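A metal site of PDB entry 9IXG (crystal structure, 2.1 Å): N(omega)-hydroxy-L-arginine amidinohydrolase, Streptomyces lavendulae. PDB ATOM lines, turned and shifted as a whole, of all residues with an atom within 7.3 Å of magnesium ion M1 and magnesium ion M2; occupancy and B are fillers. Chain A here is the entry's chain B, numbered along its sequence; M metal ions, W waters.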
ATOM      1  N   MET A  18     -16.516 -21.121 -17.003  1.00  0.00           N
ATOM      2  CA  MET A  18     -15.935 -20.081 -17.837  1.00  0.00           C
ATOM      3  C   MET A  18     -14.419 -20.211 -17.921  1.00  0.00           C
ATOM      4  O   MET A  18     -13.834 -19.855 -18.957  1.00  0.00           O
ATOM      5  CB  MET A  18     -16.396 -18.714 -17.330  1.00  0.00           C
ATOM      6  CG  MET A  18     -17.854 -18.403 -17.797  1.00  0.00           C
ATOM      7  SD  MET A  18     -18.465 -16.784 -17.358  1.00  0.00           S
ATOM      8  CE  MET A  18     -18.206 -16.920 -15.588  1.00  0.00           C
ATOM      9  N   THR A  85     -13.466 -14.409 -17.716  1.00  0.00           N
ATOM     10  CA  THR A  85     -14.492 -13.394 -17.483  1.00  0.00           C
ATOM     11  C   THR A  85     -14.057 -12.031 -18.017  1.00  0.00           C
ATOM     12  O   THR A  85     -12.858 -11.754 -18.148  1.00  0.00           O
ATOM     13  CB  THR A  85     -14.848 -13.253 -15.988  1.00  0.00           C
ATOM     14  OG1 THR A  85     -13.682 -12.841 -15.258  1.00  0.00           O
ATOM     15  CG2 THR A  85     -15.354 -14.570 -15.413  1.00  0.00           C
ATOM     16  N   CYS A  86     -15.055 -11.167 -18.293  1.00  0.00           N
ATOM     17  CA  CYS A  86     -14.774  -9.782 -18.671  1.00  0.00           C
ATOM     18  C   CYS A  86     -13.966  -9.040 -17.595  1.00  0.00           C
ATOM     19  O   CYS A  86     -13.279  -8.062 -17.911  1.00  0.00           O
ATOM     20  CB  CYS A  86     -16.069  -8.999 -18.940  1.00  0.00           C
ATOM     21  SG  CYS A  86     -16.901  -9.144 -20.608  1.00  0.00           S
ATOM     22  N   SER A  87     -14.042  -9.469 -16.346  1.00  0.00           N
ATOM     23  CA  SER A  87     -13.382  -8.701 -15.281  1.00  0.00           C
ATOM     24  C   SER A  87     -11.869  -8.739 -15.393  1.00  0.00           C
ATOM     25  O   SER A  87     -11.197  -7.891 -14.799  1.00  0.00           O
ATOM     26  CB  SER A  87     -13.816  -9.219 -13.902  1.00  0.00           C
ATOM     27  OG  SER A  87     -15.226  -9.129 -13.745  1.00  0.00           O
ATOM     28  N   TYR A 107     -16.063  -2.351 -27.472  1.00  0.00           N
ATOM     29  CA  TYR A 107     -16.506  -3.170 -26.353  1.00  0.00           C
ATOM     30  C   TYR A 107     -17.787  -3.835 -26.814  1.00  0.00           C
ATOM     31  O   TYR A 107     -18.882  -3.284 -26.655  1.00  0.00           O
ATOM     32  CB  TYR A 107     -16.695  -2.333 -25.083  1.00  0.00           C
ATOM     33  CG  TYR A 107     -16.691  -3.156 -23.829  1.00  0.00           C
ATOM     34  CD1 TYR A 107     -17.860  -3.764 -23.380  1.00  0.00           C
ATOM     35  CD2 TYR A 107     -15.540  -3.310 -23.084  1.00  0.00           C
ATOM     36  CE1 TYR A 107     -17.864  -4.530 -22.217  1.00  0.00           C
ATOM     37  CE2 TYR A 107     -15.524  -4.076 -21.927  1.00  0.00           C
ATOM     38  CZ  TYR A 107     -16.689  -4.679 -21.498  1.00  0.00           C
ATOM     39  OH  TYR A 107     -16.677  -5.419 -20.356  1.00  0.00           O
ATOM     40  N   ILE A 108     -17.651  -5.023 -27.377  1.00  0.00           N
ATOM     41  CA  ILE A 108     -18.746  -5.735 -28.026  1.00  0.00           C
ATOM     42  C   ILE A 108     -19.392  -6.638 -26.989  1.00  0.00           C
ATOM     43  O   ILE A 108     -18.826  -7.652 -26.562  1.00  0.00           O
ATOM     44  CB  ILE A 108     -18.242  -6.520 -29.243  1.00  0.00           C
ATOM     45  CG1 ILE A 108     -17.357  -5.613 -30.108  1.00  0.00           C
ATOM     46  CG2 ILE A 108     -19.408  -7.025 -30.050  1.00  0.00           C
ATOM     47  CD1 ILE A 108     -16.954  -6.211 -31.441  1.00  0.00           C
ATOM     48  N   ASP A 109     -20.593  -6.258 -26.558  1.00  0.00           N
ATOM     49  CA  ASP A 109     -21.138  -6.753 -25.299  1.00  0.00           C
ATOM     50  C   ASP A 109     -22.643  -6.568 -25.304  1.00  0.00           C
ATOM     51  O   ASP A 109     -23.140  -5.547 -25.779  1.00  0.00           O
ATOM     52  CB  ASP A 109     -20.472  -5.991 -24.140  1.00  0.00           C
ATOM     53  CG  ASP A 109     -20.772  -6.589 -22.778  1.00  0.00           C
ATOM     54  OD1 ASP A 109     -21.774  -6.187 -22.156  1.00  0.00           O
ATOM     55  OD2 ASP A 109     -19.952  -7.442 -22.334  1.00  0.00           O
ATOM     56  N   GLY A 110     -23.383  -7.565 -24.793  1.00  0.00           N
ATOM     57  CA  GLY A 110     -24.825  -7.411 -24.710  1.00  0.00           C
ATOM     58  C   GLY A 110     -25.340  -6.473 -23.623  1.00  0.00           C
ATOM     59  O   GLY A 110     -26.523  -6.103 -23.643  1.00  0.00           O
ATOM     60  N   HIS A 111     -24.493  -6.062 -22.680  1.00  0.00           N
ATOM     61  CA  HIS A 111     -24.972  -5.355 -21.489  1.00  0.00           C
ATOM     62  C   HIS A 111     -24.463  -3.939 -21.343  1.00  0.00           C
ATOM     63  O   HIS A 111     -25.205  -3.066 -20.884  1.00  0.00           O
ATOM     64  CB  HIS A 111     -24.598  -6.133 -20.215  1.00  0.00           C
ATOM     65  CG  HIS A 111     -25.358  -7.401 -20.065  1.00  0.00           C
ATOM     66  ND1 HIS A 111     -26.585  -7.460 -19.440  1.00  0.00           N
ATOM     67  CD2 HIS A 111     -25.093  -8.664 -20.476  1.00  0.00           C
ATOM     68  CE1 HIS A 111     -27.031  -8.700 -19.454  1.00  0.00           C
ATOM     69  NE2 HIS A 111     -26.144  -9.454 -20.085  1.00  0.00           N
ATOM     70  N   GLY A 112     -23.197  -3.680 -21.655  1.00  0.00           N
ATOM     71  CA  GLY A 112     -22.583  -2.381 -21.426  1.00  0.00           C
ATOM     72  C   GLY A 112     -21.547  -2.365 -20.321  1.00  0.00           C
ATOM     73  O   GLY A 112     -20.588  -1.594 -20.397  1.00  0.00           O
ATOM     74  N   ASP A 113     -21.745  -3.176 -19.269  1.00  0.00           N
ATOM     75  CA  ASP A 113     -20.739  -3.347 -18.198  1.00  0.00           C
ATOM     76  C   ASP A 113     -20.251  -2.003 -17.644  1.00  0.00           C
ATOM     77  O   ASP A 113     -19.056  -1.789 -17.403  1.00  0.00           O
ATOM     78  CB  ASP A 113     -19.559  -4.196 -18.695  1.00  0.00           C
ATOM     79  CG  ASP A 113     -19.977  -5.624 -19.048  1.00  0.00           C
ATOM     80  OD1 ASP A 113     -21.060  -6.033 -18.593  1.00  0.00           O
ATOM     81  OD2 ASP A 113     -19.217  -6.329 -19.743  1.00  0.00           O
ATOM     82  N   TYR A 124     -22.166  -7.579  -9.253  1.00  0.00           N
ATOM     83  CA  TYR A 124     -21.294  -8.346 -10.132  1.00  0.00           C
ATOM     84  C   TYR A 124     -20.198  -7.460 -10.731  1.00  0.00           C
ATOM     85  O   TYR A 124     -20.467  -6.564 -11.533  1.00  0.00           O
ATOM     86  CB  TYR A 124     -22.110  -9.017 -11.233  1.00  0.00           C
ATOM     87  CG  TYR A 124     -21.278  -9.898 -12.140  1.00  0.00           C
ATOM     88  CD1 TYR A 124     -20.330 -10.756 -11.609  1.00  0.00           C
ATOM     89  CD2 TYR A 124     -21.462  -9.889 -13.519  1.00  0.00           C
ATOM     90  CE1 TYR A 124     -19.565 -11.572 -12.428  1.00  0.00           C
ATOM     91  CE2 TYR A 124     -20.708 -10.714 -14.341  1.00  0.00           C
ATOM     92  CZ  TYR A 124     -19.748 -11.537 -13.789  1.00  0.00           C
ATOM     93  OH  TYR A 124     -18.970 -12.373 -14.579  1.00  0.00           O
ATOM     94  N   GLY A 126     -18.216  -8.206 -13.025  1.00  0.00           N
ATOM     95  CA  GLY A 126     -18.262  -8.315 -14.472  1.00  0.00           C
ATOM     96  C   GLY A 126     -19.113  -7.253 -15.130  1.00  0.00           C
ATOM     97  O   GLY A 126     -18.919  -6.953 -16.328  1.00  0.00           O
ATOM     98  N   GLY A 127     -20.059  -6.677 -14.399  1.00  0.00           N
ATOM     99  CA  GLY A 127     -20.804  -5.546 -14.892  1.00  0.00           C
ATOM    100  C   GLY A 127     -20.201  -4.188 -14.607  1.00  0.00           C
ATOM    101  O   GLY A 127     -20.859  -3.171 -14.830  1.00  0.00           O
ATOM    102  N   VAL A 129     -16.763  -3.334 -15.591  1.00  0.00           N
ATOM    103  CA  VAL A 129     -15.435  -3.414 -16.202  1.00  0.00           C
ATOM    104  C   VAL A 129     -15.107  -2.139 -16.979  1.00  0.00           C
ATOM    105  O   VAL A 129     -14.046  -1.525 -16.784  1.00  0.00           O
ATOM    106  CB  VAL A 129     -15.344  -4.656 -17.114  1.00  0.00           C
ATOM    107  CG1 VAL A 129     -14.112  -4.605 -18.045  1.00  0.00           C
ATOM    108  CG2 VAL A 129     -15.363  -5.913 -16.273  1.00  0.00           C
ATOM    109  N   HIS A 196     -12.798  -5.971 -27.698  1.00  0.00           N
ATOM    110  CA  HIS A 196     -13.203  -6.788 -26.561  1.00  0.00           C
ATOM    111  C   HIS A 196     -14.556  -7.396 -26.905  1.00  0.00           C
ATOM    112  O   HIS A 196     -15.489  -6.666 -27.246  1.00  0.00           O
ATOM    113  CB  HIS A 196     -13.286  -5.928 -25.297  1.00  0.00           C
ATOM    114  CG  HIS A 196     -13.934  -6.617 -24.130  1.00  0.00           C
ATOM    115  ND1 HIS A 196     -13.244  -6.936 -22.990  1.00  0.00           N
ATOM    116  CD2 HIS A 196     -15.212  -7.030 -23.935  1.00  0.00           C
ATOM    117  CE1 HIS A 196     -14.067  -7.525 -22.124  1.00  0.00           C
ATOM    118  NE2 HIS A 196     -15.267  -7.599 -22.676  1.00  0.00           N
ATOM    119  N   ILE A 197     -14.683  -8.703 -26.855  1.00  0.00           N
ATOM    120  CA  ILE A 197     -15.983  -9.310 -27.147  1.00  0.00           C
ATOM    121  C   ILE A 197     -16.403 -10.266 -26.029  1.00  0.00           C
ATOM    122  O   ILE A 197     -15.633 -11.146 -25.622  1.00  0.00           O
ATOM    123  CB  ILE A 197     -16.004 -10.004 -28.524  1.00  0.00           C
ATOM    124  CG1 ILE A 197     -17.421 -10.523 -28.835  1.00  0.00           C
ATOM    125  CG2 ILE A 197     -14.956 -11.080 -28.621  1.00  0.00           C
ATOM    126  CD1 ILE A 197     -17.685 -10.616 -30.309  1.00  0.00           C
ATOM    127  N   ASP A 198     -17.618 -10.070 -25.534  1.00  0.00           N
ATOM    128  CA  ASP A 198     -18.297 -10.937 -24.578  1.00  0.00           C
ATOM    129  C   ASP A 198     -19.403 -11.653 -25.356  1.00  0.00           C
ATOM    130  O   ASP A 198     -20.242 -11.007 -25.985  1.00  0.00           O
ATOM    131  CB  ASP A 198     -18.833 -10.080 -23.421  1.00  0.00           C
ATOM    132  CG  ASP A 198     -19.701 -10.849 -22.422  1.00  0.00           C
ATOM    133  OD1 ASP A 198     -20.069 -12.031 -22.627  1.00  0.00           O
ATOM    134  OD2 ASP A 198     -20.026 -10.237 -21.385  1.00  0.00           O
ATOM    135  N   TRP A 199     -19.351 -12.988 -25.374  1.00  0.00           N
ATOM    136  CA  TRP A 199     -20.267 -13.743 -26.221  1.00  0.00           C
ATOM    137  C   TRP A 199     -21.732 -13.535 -25.876  1.00  0.00           C
ATOM    138  O   TRP A 199     -22.592 -13.994 -26.644  1.00  0.00           O
ATOM    139  CB  TRP A 199     -19.909 -15.228 -26.169  1.00  0.00           C
ATOM    140  CG  TRP A 199     -18.496 -15.444 -26.579  1.00  0.00           C
ATOM    141  CD1 TRP A 199     -17.494 -16.041 -25.843  1.00  0.00           C
ATOM    142  CD2 TRP A 199     -17.893 -15.006 -27.800  1.00  0.00           C
ATOM    143  NE1 TRP A 199     -16.321 -16.027 -26.553  1.00  0.00           N
ATOM    144  CE2 TRP A 199     -16.534 -15.409 -27.755  1.00  0.00           C
ATOM    145  CE3 TRP A 199     -18.377 -14.361 -28.941  1.00  0.00           C
ATOM    146  CZ2 TRP A 199     -15.645 -15.150 -28.801  1.00  0.00           C
ATOM    147  CZ3 TRP A 199     -17.488 -14.112 -29.989  1.00  0.00           C
ATOM    148  CH2 TRP A 199     -16.135 -14.505 -29.901  1.00  0.00           C
ATOM    149  N   ASP A 200     -22.057 -12.847 -24.776  1.00  0.00           N
ATOM    150  CA  ASP A 200     -23.443 -12.519 -24.510  1.00  0.00           C
ATOM    151  C   ASP A 200     -24.015 -11.504 -25.495  1.00  0.00           C
ATOM    152  O   ASP A 200     -25.240 -11.357 -25.562  1.00  0.00           O
ATOM    153  CB  ASP A 200     -23.624 -12.077 -23.028  1.00  0.00           C
ATOM    154  CG  ASP A 200     -22.943 -10.736 -22.670  1.00  0.00           C
ATOM    155  OD1 ASP A 200     -22.789  -9.846 -23.508  1.00  0.00           O
ATOM    156  OD2 ASP A 200     -22.595 -10.561 -21.474  1.00  0.00           O
ATOM    157  N   VAL A 201     -23.181 -10.823 -26.282  1.00  0.00           N
ATOM    158  CA  VAL A 201     -23.678  -9.948 -27.343  1.00  0.00           C
ATOM    159  C   VAL A 201     -24.482 -10.699 -28.389  1.00  0.00           C
ATOM    160  O   VAL A 201     -25.293 -10.085 -29.095  1.00  0.00           O
ATOM    161  CB  VAL A 201     -22.499  -9.191 -27.992  1.00  0.00           C
ATOM    162  CG1 VAL A 201     -21.699 -10.120 -28.939  1.00  0.00           C
ATOM    163  CG2 VAL A 201     -22.979  -7.943 -28.719  1.00  0.00           C
ATOM    164  N   ALA A 209     -23.542 -18.640 -22.850  1.00  0.00           N
ATOM    165  CA  ALA A 209     -22.991 -17.610 -21.978  1.00  0.00           C
ATOM    166  C   ALA A 209     -24.014 -17.293 -20.899  1.00  0.00           C
ATOM    167  O   ALA A 209     -25.231 -17.359 -21.137  1.00  0.00           O
ATOM    168  CB  ALA A 209     -22.632 -16.336 -22.761  1.00  0.00           C
ATOM    169  N   ASP A 210     -23.539 -16.931 -19.704  1.00  0.00           N
ATOM    170  CA  ASP A 210     -24.467 -16.436 -18.696  1.00  0.00           C
ATOM    171  C   ASP A 210     -24.868 -14.999 -19.043  1.00  0.00           C
ATOM    172  O   ASP A 210     -24.290 -14.345 -19.917  1.00  0.00           O
ATOM    173  CB  ASP A 210     -23.863 -16.542 -17.285  1.00  0.00           C
ATOM    174  CG  ASP A 210     -22.580 -15.717 -17.096  1.00  0.00           C
ATOM    175  OD1 ASP A 210     -21.969 -15.287 -18.108  1.00  0.00           O
ATOM    176  OD2 ASP A 210     -22.182 -15.499 -15.922  1.00  0.00           O
ATOM    177  N   TYR A 211     -25.930 -14.523 -18.371  1.00  0.00           N
ATOM    178  CA  TYR A 211     -26.444 -13.158 -18.579  1.00  0.00           C
ATOM    179  C   TYR A 211     -26.894 -12.947 -20.039  1.00  0.00           C
ATOM    180  O   TYR A 211     -26.551 -11.949 -20.688  1.00  0.00           O
ATOM    181  CB  TYR A 211     -25.391 -12.115 -18.166  1.00  0.00           C
ATOM    182  CG  TYR A 211     -25.137 -12.060 -16.663  1.00  0.00           C
ATOM    183  CD1 TYR A 211     -26.029 -11.407 -15.817  1.00  0.00           C
ATOM    184  CD2 TYR A 211     -24.008 -12.654 -16.091  1.00  0.00           C
ATOM    185  CE1 TYR A 211     -25.804 -11.335 -14.441  1.00  0.00           C
ATOM    186  CE2 TYR A 211     -23.773 -12.593 -14.716  1.00  0.00           C
ATOM    187  CZ  TYR A 211     -24.680 -11.930 -13.902  1.00  0.00           C
ATOM    188  OH  TYR A 211     -24.473 -11.853 -12.538  1.00  0.00           O
ATOM    189  N   THR A 212     -27.667 -13.914 -20.547  1.00  0.00           N
ATOM    190  CA  THR A 212     -28.230 -13.890 -21.899  1.00  0.00           C
ATOM    191  C   THR A 212     -29.257 -12.764 -22.026  1.00  0.00           C
ATOM    192  O   THR A 212     -29.974 -12.447 -21.079  1.00  0.00           O
ATOM    193  CB  THR A 212     -28.890 -15.238 -22.203  1.00  0.00           C
ATOM    194  OG1 THR A 212     -27.915 -16.290 -22.140  1.00  0.00           O
ATOM    195  CG2 THR A 212     -29.500 -15.262 -23.556  1.00  0.00           C
ATOM    196  N   ALA A 240     -14.051 -13.518 -24.395  1.00  0.00           N
ATOM    197  CA  ALA A 240     -14.439 -13.757 -23.018  1.00  0.00           C
ATOM    198  C   ALA A 240     -15.805 -14.408 -22.913  1.00  0.00           C
ATOM    199  O   ALA A 240     -16.724 -14.070 -23.681  1.00  0.00           O
ATOM    200  CB  ALA A 240     -14.455 -12.444 -22.199  1.00  0.00           C
ATOM    201  N   GLU A 241     -15.921 -15.317 -21.945  1.00  0.00           N
ATOM    202  CA  GLU A 241     -17.171 -15.731 -21.272  1.00  0.00           C
ATOM    203  C   GLU A 241     -17.908 -16.848 -22.002  1.00  0.00           C
ATOM    204  O   GLU A 241     -19.148 -16.854 -22.039  1.00  0.00           O
ATOM    205  CB  GLU A 241     -18.112 -14.537 -21.038  1.00  0.00           C
ATOM    206  CG  GLU A 241     -17.438 -13.371 -20.317  1.00  0.00           C
ATOM    207  CD  GLU A 241     -18.279 -12.756 -19.241  1.00  0.00           C
ATOM    208  OE1 GLU A 241     -17.698 -12.267 -18.233  1.00  0.00           O
ATOM    209  OE2 GLU A 241     -19.528 -12.738 -19.399  1.00  0.00           O
HETATM  210 MG    MG M   1     -19.485  -8.306 -20.413  1.00  0.00          MG
HETATM  211 MG    MG M   2     -21.061 -11.843 -20.472  1.00  0.00          MG
HETATM  212  O   HOH W   1     -19.135  -8.962 -18.343  1.00  0.00           O
HETATM  213  O   HOH W   2     -21.926 -13.885 -20.431  1.00  0.00           O
HETATM  214  O   HOH W   3     -21.784  -8.469 -20.197  1.00  0.00           O
HETATM  215  O   HOH W   4     -21.300 -11.045 -18.643  1.00  0.00           O
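Water W3 bridges OD1 of Asp 113 and OD1 of Asp 109.
Magnesium ion M1 is bound by the side-chain carboxylate of Asp 113 (2.1 Å), the side-chain carboxylate of Asp 109 (2.2 Å), water W1 (2.2 Å), the side-chain carboxylate of Asp 198 (2.2 Å), water W3 (2.3 Å) and the side-chain sulfur of Cys 86 (2.7 Å).
Within 4 Å of magnesium ion M1: Cys 86, Asp 109, Asp 113, Asp 198 and Asp 200. The nearest printed residue that does not touch magnesium ion M1 is Tyr 107 (4.03 Å).
O of Asp 113 sits at hydrogen-bond distance from N of Val 129 (3.3 Å). SG of Cys 86 sits close to OH of Tyr 107. The backbone NH (N) of Gly 110 lies within hydrogen-bond range of the side-chain carboxylate (OD1) of Asp 200, 2.7 Å away. The backbone NH of Asp 198 is in hydrogen-bond range of the backbone carbonyl oxygen of Ile 108 (2.9 Å). N of Cys 86 sits at hydrogen-bond distance from OE1 of Glu 241. The side-chain carboxylate (OD1) of Asp 109 lies within hydrogen-bond range of the backbone NH (N) of Gly 112 (2.9 Å). The backbone NH (N) of His 111 lies within hydrogen-bond range of the side-chain carboxylate (OD1) of Asp 109 (2.8 Å). The side-chain sulfur of Cys 86 lies close to a ring nitrogen (NE2) of His 196, 3.1 Å away.
Magnesium ion M2 is bound by water W4 (2.0 Å), the side-chain carboxylate (OE2) of Glu 241 (2.1 Å), the side-chain carboxylate (OD2) of Asp 198 (2.1 Å), water W2 (2.2 Å), the side-chain carboxylate (OD2) of Asp 200 (2.2 Å) and the side-chain carboxylate (OD1) of Asp 198 (2.4 Å). Magnesium ion M2 has six donor atoms within binding distance.
Of the 27 residues printed, 3 come within 4 Å of magnesium ion M2. The nearest printed residue that does not touch magnesium ion M2 is Asp 210 (4.1 Å).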
